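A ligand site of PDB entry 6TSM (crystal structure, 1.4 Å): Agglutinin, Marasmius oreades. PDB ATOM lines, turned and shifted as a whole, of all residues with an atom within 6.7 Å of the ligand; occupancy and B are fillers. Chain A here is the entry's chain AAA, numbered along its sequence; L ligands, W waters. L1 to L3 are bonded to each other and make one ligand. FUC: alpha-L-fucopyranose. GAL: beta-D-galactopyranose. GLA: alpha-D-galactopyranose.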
ATOM      1  N   HIS A   9     -29.037  -2.341  27.619  1.00  0.00           N
ATOM      2  CA  HIS A   9     -29.635  -1.032  27.317  1.00  0.00           C
ATOM      3  C   HIS A   9     -31.140  -1.206  27.149  1.00  0.00           C
ATOM      4  O   HIS A   9     -31.526  -2.017  26.322  1.00  0.00           O
ATOM      5  CB  HIS A   9     -29.000  -0.457  26.066  1.00  0.00           C
ATOM      6  CG  HIS A   9     -29.287   0.993  25.832  1.00  0.00           C
ATOM      7  ND1 HIS A   9     -30.029   1.445  24.751  1.00  0.00           N
ATOM      8  CD2 HIS A   9     -29.012   2.089  26.579  1.00  0.00           C
ATOM      9  CE1 HIS A   9     -30.148   2.757  24.819  1.00  0.00           C
ATOM     10  NE2 HIS A   9     -29.522   3.178  25.907  1.00  0.00           N
ATOM     11  N   ASP A  20     -32.831   5.586  32.196  1.00  0.00           N
ATOM     12  CA  ASP A  20     -31.673   6.457  32.423  1.00  0.00           C
ATOM     13  C   ASP A  20     -31.614   6.797  33.908  1.00  0.00           C
ATOM     14  O   ASP A  20     -32.630   7.253  34.445  1.00  0.00           O
ATOM     15  CB  ASP A  20     -31.757   7.701  31.536  1.00  0.00           C
ATOM     16  CG  ASP A  20     -30.571   8.642  31.606  1.00  0.00           C
ATOM     17  OD1 ASP A  20     -30.360   9.194  32.673  1.00  0.00           O
ATOM     18  OD2 ASP A  20     -29.954   8.906  30.521  1.00  0.00           O
ATOM     19  N   LEU A  21     -30.497   6.552  34.548  1.00  0.00           N
ATOM     20  CA  LEU A  21     -30.282   7.078  35.919  1.00  0.00           C
ATOM     21  C   LEU A  21     -29.834   8.527  35.817  1.00  0.00           C
ATOM     22  O   LEU A  21     -28.691   8.769  35.313  1.00  0.00           O
ATOM     23  CB  LEU A  21     -29.224   6.238  36.633  1.00  0.00           C
ATOM     24  CG  LEU A  21     -28.920   6.655  38.089  1.00  0.00           C
ATOM     25  CD1 LEU A  21     -30.142   6.540  38.964  1.00  0.00           C
ATOM     26  CD2 LEU A  21     -27.782   5.827  38.658  1.00  0.00           C
ATOM     27  N   LYS A  22     -30.652   9.463  36.291  1.00  0.00           N
ATOM     28  CA  LYS A  22     -30.475  10.888  35.937  1.00  0.00           C
ATOM     29  C   LYS A  22     -29.072  11.363  36.404  1.00  0.00           C
ATOM     30  O   LYS A  22     -28.751  11.232  37.615  1.00  0.00           O
ATOM     31  CB  LYS A  22     -31.580  11.759  36.528  1.00  0.00           C
ATOM     32  CG  LYS A  22     -31.781  13.061  35.803  1.00  0.00           C
ATOM     33  CD  LYS A  22     -32.968  13.863  36.237  1.00  0.00           C
ATOM     34  CE  LYS A  22     -33.066  15.178  35.480  1.00  0.00           C
ATOM     35  NZ  LYS A  22     -34.380  15.846  35.697  1.00  0.00           N
ATOM     36  N   ASP A  23     -28.310  11.934  35.466  1.00  0.00           N
ATOM     37  CA  ASP A  23     -26.946  12.497  35.677  1.00  0.00           C
ATOM     38  C   ASP A  23     -25.981  11.394  36.185  1.00  0.00           C
ATOM     39  O   ASP A  23     -24.869  11.746  36.594  1.00  0.00           O
ATOM     40  CB  ASP A  23     -26.987  13.669  36.640  1.00  0.00           C
ATOM     41  CG  ASP A  23     -25.841  14.642  36.429  1.00  0.00           C
ATOM     42  OD1 ASP A  23     -25.397  14.788  35.278  1.00  0.00           O
ATOM     43  OD2 ASP A  23     -25.330  15.161  37.444  1.00  0.00           O
ATOM     44  N   GLY A  24     -26.385  10.141  36.122  1.00  0.00           N
ATOM     45  CA  GLY A  24     -25.556   9.025  36.589  1.00  0.00           C
ATOM     46  C   GLY A  24     -25.300   9.088  38.105  1.00  0.00           C
ATOM     47  O   GLY A  24     -24.335   8.484  38.563  1.00  0.00           O
ATOM     48  N   VAL A  33     -35.390   7.777  34.806  1.00  0.00           N
ATOM     49  CA  VAL A  33     -36.236   8.557  33.880  1.00  0.00           C
ATOM     50  C   VAL A  33     -36.069   7.981  32.456  1.00  0.00           C
ATOM     51  O   VAL A  33     -35.049   7.334  32.183  1.00  0.00           O
ATOM     52  CB  VAL A  33     -35.869  10.047  33.915  1.00  0.00           C
ATOM     53  CG1 VAL A  33     -36.159  10.667  35.273  1.00  0.00           C
ATOM     54  CG2 VAL A  33     -34.421  10.286  33.518  1.00  0.00           C
ATOM     55  N   TRP A  35     -35.072   8.730  28.630  1.00  0.00           N
ATOM     56  CA  TRP A  35     -34.130   9.681  27.983  1.00  0.00           C
ATOM     57  C   TRP A  35     -33.770   9.165  26.606  1.00  0.00           C
ATOM     58  O   TRP A  35     -33.595   7.955  26.450  1.00  0.00           O
ATOM     59  CB  TRP A  35     -32.866   9.881  28.868  1.00  0.00           C
ATOM     60  CG  TRP A  35     -32.191  11.197  28.670  1.00  0.00           C
ATOM     61  CD1 TRP A  35     -31.404  11.575  27.629  1.00  0.00           C
ATOM     62  CD2 TRP A  35     -32.284  12.344  29.538  1.00  0.00           C
ATOM     63  NE1 TRP A  35     -30.989  12.885  27.794  1.00  0.00           N
ATOM     64  CE2 TRP A  35     -31.532  13.385  28.945  1.00  0.00           C
ATOM     65  CE3 TRP A  35     -32.973  12.602  30.739  1.00  0.00           C
ATOM     66  CZ2 TRP A  35     -31.452  14.651  29.517  1.00  0.00           C
ATOM     67  CZ3 TRP A  35     -32.875  13.846  31.311  1.00  0.00           C
ATOM     68  CH2 TRP A  35     -32.131  14.861  30.698  1.00  0.00           C
ATOM     69  N   GLN A  36     -33.534  10.041  25.678  1.00  0.00           N
ATOM     70  CA  GLN A  36     -33.145   9.625  24.312  1.00  0.00           C
ATOM     71  C   GLN A  36     -31.696   9.097  24.328  1.00  0.00           C
ATOM     72  O   GLN A  36     -30.972   9.332  25.313  1.00  0.00           O
ATOM     73  CB  GLN A  36     -33.292  10.797  23.316  1.00  0.00           C
ATOM     74  CG  GLN A  36     -32.361  11.949  23.546  1.00  0.00           C
ATOM     75  CD  GLN A  36     -32.528  13.031  22.500  1.00  0.00           C
ATOM     76  OE1 GLN A  36     -32.326  12.808  21.309  1.00  0.00           O
ATOM     77  NE2 GLN A  36     -32.998  14.177  22.931  1.00  0.00           N
ATOM     78  N   PHE A  37     -31.299   8.427  23.265  1.00  0.00           N
ATOM     79  CA  PHE A  37     -30.021   7.709  23.251  1.00  0.00           C
ATOM     80  C   PHE A  37     -29.443   7.738  21.842  1.00  0.00           C
ATOM     81  O   PHE A  37     -30.136   8.119  20.907  1.00  0.00           O
ATOM     82  CB  PHE A  37     -30.219   6.275  23.767  1.00  0.00           C
ATOM     83  CG  PHE A  37     -31.236   5.461  23.008  1.00  0.00           C
ATOM     84  CD1 PHE A  37     -30.855   4.685  21.916  1.00  0.00           C
ATOM     85  CD2 PHE A  37     -32.549   5.381  23.440  1.00  0.00           C
ATOM     86  CE1 PHE A  37     -31.787   3.904  21.252  1.00  0.00           C
ATOM     87  CE2 PHE A  37     -33.470   4.591  22.766  1.00  0.00           C
ATOM     88  CZ  PHE A  37     -33.086   3.854  21.684  1.00  0.00           C
ATOM     89  N   THR A  38     -28.161   7.495  21.751  1.00  0.00           N
ATOM     90  CA  THR A  38     -27.460   7.395  20.453  1.00  0.00           C
ATOM     91  C   THR A  38     -27.001   5.953  20.257  1.00  0.00           C
ATOM     92  O   THR A  38     -26.166   5.470  20.995  1.00  0.00           O
ATOM     93  CB  THR A  38     -26.286   8.373  20.379  1.00  0.00           C
ATOM     94  OG1 THR A  38     -26.753   9.670  20.826  1.00  0.00           O
ATOM     95  CG2 THR A  38     -25.703   8.479  18.991  1.00  0.00           C
ATOM     96  N   PRO A  39     -27.528   5.245  19.256  1.00  0.00           N
ATOM     97  CA  PRO A  39     -27.057   3.878  18.964  1.00  0.00           C
ATOM     98  C   PRO A  39     -25.559   3.854  18.613  1.00  0.00           C
ATOM     99  O   PRO A  39     -25.070   4.840  18.092  1.00  0.00           O
ATOM    100  CB  PRO A  39     -27.899   3.442  17.737  1.00  0.00           C
ATOM    101  CG  PRO A  39     -29.099   4.419  17.729  1.00  0.00           C
ATOM    102  CD  PRO A  39     -28.560   5.702  18.339  1.00  0.00           C
ATOM    103  N   THR A  41     -22.993   3.945  20.500  1.00  0.00           N
ATOM    104  CA  THR A  41     -22.158   4.634  21.466  1.00  0.00           C
ATOM    105  C   THR A  41     -22.230   3.895  22.793  1.00  0.00           C
ATOM    106  O   THR A  41     -23.182   3.076  22.968  1.00  0.00           O
ATOM    107  CB  THR A  41     -22.584   6.104  21.667  1.00  0.00           C
ATOM    108  OG1 THR A  41     -23.857   6.131  22.360  1.00  0.00           O
ATOM    109  CG2 THR A  41     -22.686   6.872  20.383  1.00  0.00           C
ATOM    110  N   ILE A  42     -21.402   4.292  23.730  1.00  0.00           N
ATOM    111  CA  ILE A  42     -21.650   4.051  25.170  1.00  0.00           C
ATOM    112  C   ILE A  42     -22.636   5.114  25.670  1.00  0.00           C
ATOM    113  O   ILE A  42     -22.282   6.327  25.623  1.00  0.00           O
ATOM    114  CB  ILE A  42     -20.341   4.077  25.961  1.00  0.00           C
ATOM    115  CG1 ILE A  42     -19.389   2.948  25.521  1.00  0.00           C
ATOM    116  CG2 ILE A  42     -20.608   4.033  27.443  1.00  0.00           C
ATOM    117  CD1 ILE A  42     -19.950   1.581  25.695  1.00  0.00           C
ATOM    118  N   ASN A  43     -23.851   4.692  26.004  1.00  0.00           N
ATOM    119  CA  ASN A  43     -24.838   5.561  26.660  1.00  0.00           C
ATOM    120  C   ASN A  43     -24.607   5.500  28.182  1.00  0.00           C
ATOM    121  O   ASN A  43     -25.096   4.533  28.835  1.00  0.00           O
ATOM    122  CB  ASN A  43     -26.273   5.196  26.252  1.00  0.00           C
ATOM    123  CG  ASN A  43     -26.549   5.532  24.794  1.00  0.00           C
ATOM    124  OD1 ASN A  43     -26.785   6.675  24.459  1.00  0.00           O
ATOM    125  ND2 ASN A  43     -26.489   4.533  23.921  1.00  0.00           N
ATOM    126  N   TRP A  44     -23.796   6.420  28.695  1.00  0.00           N
ATOM    127  CA  TRP A  44     -23.078   6.281  29.974  1.00  0.00           C
ATOM    128  C   TRP A  44     -24.045   6.027  31.133  1.00  0.00           C
ATOM    129  O   TRP A  44     -23.622   5.382  32.110  1.00  0.00           O
ATOM    130  CB  TRP A  44     -22.231   7.537  30.216  1.00  0.00           C
ATOM    131  CG  TRP A  44     -20.953   7.532  29.476  1.00  0.00           C
ATOM    132  CD1 TRP A  44     -20.691   8.062  28.238  1.00  0.00           C
ATOM    133  CD2 TRP A  44     -19.784   6.795  29.842  1.00  0.00           C
ATOM    134  NE1 TRP A  44     -19.427   7.758  27.860  1.00  0.00           N
ATOM    135  CE2 TRP A  44     -18.839   6.974  28.819  1.00  0.00           C
ATOM    136  CE3 TRP A  44     -19.459   5.994  30.925  1.00  0.00           C
ATOM    137  CZ2 TRP A  44     -17.561   6.431  28.889  1.00  0.00           C
ATOM    138  CZ3 TRP A  44     -18.190   5.462  30.995  1.00  0.00           C
ATOM    139  CH2 TRP A  44     -17.266   5.660  29.981  1.00  0.00           C
ATOM    140  N   HIS A  45     -25.234   6.644  31.117  1.00  0.00           N
ATOM    141  CA  HIS A  45     -26.158   6.566  32.309  1.00  0.00           C
ATOM    142  C   HIS A  45     -27.262   5.537  32.081  1.00  0.00           C
ATOM    143  O   HIS A  45     -28.148   5.446  32.950  1.00  0.00           O
ATOM    144  CB  HIS A  45     -26.738   7.943  32.625  1.00  0.00           C
ATOM    145  CG  HIS A  45     -25.708   8.993  32.827  1.00  0.00           C
ATOM    146  ND1 HIS A  45     -25.982  10.333  32.656  1.00  0.00           N
ATOM    147  CD2 HIS A  45     -24.429   8.921  33.277  1.00  0.00           C
ATOM    148  CE1 HIS A  45     -24.892  11.046  32.910  1.00  0.00           C
ATOM    149  NE2 HIS A  45     -23.932  10.226  33.283  1.00  0.00           N
ATOM    150  N   GLN A  46     -27.143   4.699  31.049  1.00  0.00           N
ATOM    151  CA  GLN A  46     -28.295   3.890  30.541  1.00  0.00           C
ATOM    152  C   GLN A  46     -27.896   2.424  30.407  1.00  0.00           C
ATOM    153  O   GLN A  46     -28.607   1.700  29.713  1.00  0.00           O
ATOM    154  CB  GLN A  46     -28.762   4.425  29.194  1.00  0.00           C
ATOM    155  CG  GLN A  46     -29.169   5.893  29.240  1.00  0.00           C
ATOM    156  CD  GLN A  46     -29.627   6.427  27.896  1.00  0.00           C
ATOM    157  OE1 GLN A  46     -29.537   5.739  26.849  1.00  0.00           O
ATOM    158  NE2 GLN A  46     -30.078   7.674  27.887  1.00  0.00           N
ATOM    159  N   PHE A  66     -22.696   2.658  35.652  1.00  0.00           N
ATOM    160  CA  PHE A  66     -21.924   3.878  35.928  1.00  0.00           C
ATOM    161  C   PHE A  66     -21.931   4.172  37.447  1.00  0.00           C
ATOM    162  O   PHE A  66     -20.853   4.365  38.000  1.00  0.00           O
ATOM    163  CB  PHE A  66     -22.495   5.054  35.132  1.00  0.00           C
ATOM    164  CG  PHE A  66     -21.738   6.346  35.294  1.00  0.00           C
ATOM    165  CD1 PHE A  66     -20.566   6.584  34.594  1.00  0.00           C
ATOM    166  CD2 PHE A  66     -22.163   7.307  36.194  1.00  0.00           C
ATOM    167  CE1 PHE A  66     -19.882   7.777  34.754  1.00  0.00           C
ATOM    168  CE2 PHE A  66     -21.443   8.483  36.371  1.00  0.00           C
ATOM    169  CZ  PHE A  66     -20.332   8.727  35.623  1.00  0.00           C
ATOM    170  N   ASP A 131     -37.095  13.989  27.372  1.00  0.00           N
ATOM    171  CA  ASP A 131     -35.894  13.702  28.196  1.00  0.00           C
ATOM    172  C   ASP A 131     -36.201  14.049  29.654  1.00  0.00           C
ATOM    173  O   ASP A 131     -36.560  15.216  29.940  1.00  0.00           O
ATOM    174  CB  ASP A 131     -34.682  14.464  27.708  1.00  0.00           C
ATOM    175  CG  ASP A 131     -34.163  13.981  26.373  1.00  0.00           C
ATOM    176  OD1 ASP A 131     -34.495  12.835  25.993  1.00  0.00           O
ATOM    177  OD2 ASP A 131     -33.521  14.772  25.688  1.00  0.00           O
HETATM  178  C1  FUC L   1     -24.267  12.539  27.623  1.00  0.00           C
HETATM  179  C2  FUC L   1     -23.496  13.532  26.767  1.00  0.00           C
HETATM  180  C3  FUC L   1     -22.513  14.328  27.609  1.00  0.00           C
HETATM  181  C4  FUC L   1     -21.650  13.406  28.441  1.00  0.00           C
HETATM  182  C5  FUC L   1     -22.513  12.466  29.273  1.00  0.00           C
HETATM  183  C6  FUC L   1     -21.698  11.523  30.076  1.00  0.00           C
HETATM  184  O2  FUC L   1     -24.414  14.417  26.134  1.00  0.00           O
HETATM  185  O3  FUC L   1     -21.675  15.164  26.745  1.00  0.00           O
HETATM  186  O4  FUC L   1     -20.771  12.624  27.595  1.00  0.00           O
HETATM  187  O5  FUC L   1     -23.356  11.696  28.381  1.00  0.00           O
HETATM  188  C1  GAL L   2     -26.188  13.484  30.486  1.00  0.00           C
HETATM  189  C2  GAL L   2     -25.926  12.535  29.330  1.00  0.00           C
HETATM  190  C3  GAL L   2     -27.210  12.104  28.661  1.00  0.00           C
HETATM  191  C4  GAL L   2     -28.223  11.592  29.671  1.00  0.00           C
HETATM  192  C5  GAL L   2     -28.382  12.646  30.797  1.00  0.00           C
HETATM  193  C6  GAL L   2     -29.401  12.238  31.883  1.00  0.00           C
HETATM  194  O1  GAL L   2     -25.020  13.669  31.169  1.00  0.00           O
HETATM  195  O2  GAL L   2     -25.086  13.226  28.389  1.00  0.00           O
HETATM  196  O3  GAL L   2     -26.896  11.106  27.646  1.00  0.00           O
HETATM  197  O4  GAL L   2     -27.807  10.323  30.219  1.00  0.00           O
HETATM  198  O5  GAL L   2     -27.115  12.886  31.404  1.00  0.00           O
HETATM  199  O6  GAL L   2     -28.837  11.287  32.773  1.00  0.00           O
HETATM  200  C1  GLA L   3     -27.896  10.693  26.849  1.00  0.00           C
HETATM  201  C2  GLA L   3     -27.444   9.710  25.749  1.00  0.00           C
HETATM  202  C3  GLA L   3     -26.694  10.464  24.659  1.00  0.00           C
HETATM  203  C4  GLA L   3     -27.553  11.627  24.174  1.00  0.00           C
HETATM  204  C5  GLA L   3     -27.895  12.509  25.366  1.00  0.00           C
HETATM  205  C6  GLA L   3     -28.724  13.717  24.985  1.00  0.00           C
HETATM  206  O2  GLA L   3     -26.609   8.719  26.290  1.00  0.00           O
HETATM  207  O3  GLA L   3     -26.394   9.583  23.593  1.00  0.00           O
HETATM  208  O4  GLA L   3     -28.738  11.160  23.546  1.00  0.00           O
HETATM  209  O5  GLA L   3     -28.656  11.719  26.274  1.00  0.00           O
HETATM  210  O6  GLA L   3     -28.981  14.550  26.148  1.00  0.00           O
HETATM  211  O   HOH W   1     -23.767   8.935  26.898  1.00  0.00           O
HETATM  212  O   HOH W   2     -31.120  16.206  26.273  1.00  0.00           O
HETATM  213  O   HOH W   3     -26.691  15.713  27.211  1.00  0.00           O
HETATM  214  O   HOH W   4     -26.429   8.243  29.084  1.00  0.00           O
HETATM  215  O   HOH W   5     -25.026  13.661  23.562  1.00  0.00           O
HETATM  216  O   HOH W   6     -21.681  10.628  25.813  1.00  0.00           O
HETATM  217  O   HOH W   7     -19.339  15.905  27.998  1.00  0.00           O
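OD2 of Asp 20 lies within hydrogen-bond range of O4 of GAL L2 (2.6 Å).
ND1 of His 45 is in hydrogen-bond range of O6 of GAL L2 (3.0 Å).
NE1 of Trp 35 lies within hydrogen-bond range of O5 of GLA L3 (3.0 Å).
An oxygen (O3) of GLA L3 lies within hydrogen-bond range of the backbone NH of Thr 38 (3.3 Å).
The side-chain amide oxygen (OD1) of Asn 43 is in hydrogen-bond range of an oxygen (O2) of GLA L3 (2.7 Å).
O of Gln 36 sits at hydrogen-bond distance from O4 of GLA L3 (3.4 Å).
An oxygen (O6) of GAL L2 sits at hydrogen-bond distance from the backbone NH of Asp 23 (2.8 Å).
O3 of GLA L3 lies within hydrogen-bond range of OG1 of Thr 38 (2.8 Å).
O of Gln 36 sits at hydrogen-bond distance from NE2 of Gln 46 (3.2 Å).
NE2 of Gln 46 is in hydrogen-bond range of OD2 of Asp 20 (2.9 Å).
The side-chain amide nitrogen (NE2) of Gln 36 sits at hydrogen-bond distance from the side-chain carboxylate (OD2) of Asp 131, 2.9 Å away.
The side-chain amide oxygen (OE1) of Gln 46 sits at hydrogen-bond distance from a ring nitrogen (NE2) of His 9 (2.7 Å).
The backbone carbonyl oxygen (O) of Thr 38 sits at hydrogen-bond distance from the side-chain hydroxyl (OG1) of Thr 41 (2.8 Å).
The backbone carbonyl oxygen (O) of His 45 is in hydrogen-bond range of the backbone NH (N) of Leu 21, 3.0 Å away.
The backbone NH of Asp 20 lies within hydrogen-bond range of the backbone carbonyl oxygen of Val 33.
The side-chain amide nitrogen (ND2) of Asn 43 is in hydrogen-bond range of the backbone carbonyl oxygen (O) of Thr 38, 3.1 Å away.
O of Leu 21 touches O6 of GAL L2, at 3.6 Å.
Lys 22 touches the ligand.
CA of Phe 37 touches O4 of GLA L3, 3.7 Å away.
NE2 of Gln 46 touches C1 of GLA L3 (3.9 Å).
Hydrophobic or aromatic side chains within 4 Å of the ligand: Trp 35 and His 45.
Of the 20 residues printed, 11 come within 4 Å of the ligand.
Water W2 bridges an oxygen (O6) of GLA L3 (2.7 Å) and the side-chain carboxylate (OD2) of Asp 131 (2.9 Å).
Water W4 lies within hydrogen-bond range of O4 of GAL L2, N of His 45 and N of Trp 44.
Water W1 lies within hydrogen-bond range of an oxygen (O2) of GLA L3, the backbone NH (N) of Trp 44 and the backbone carbonyl oxygen (O) of Ile 42.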
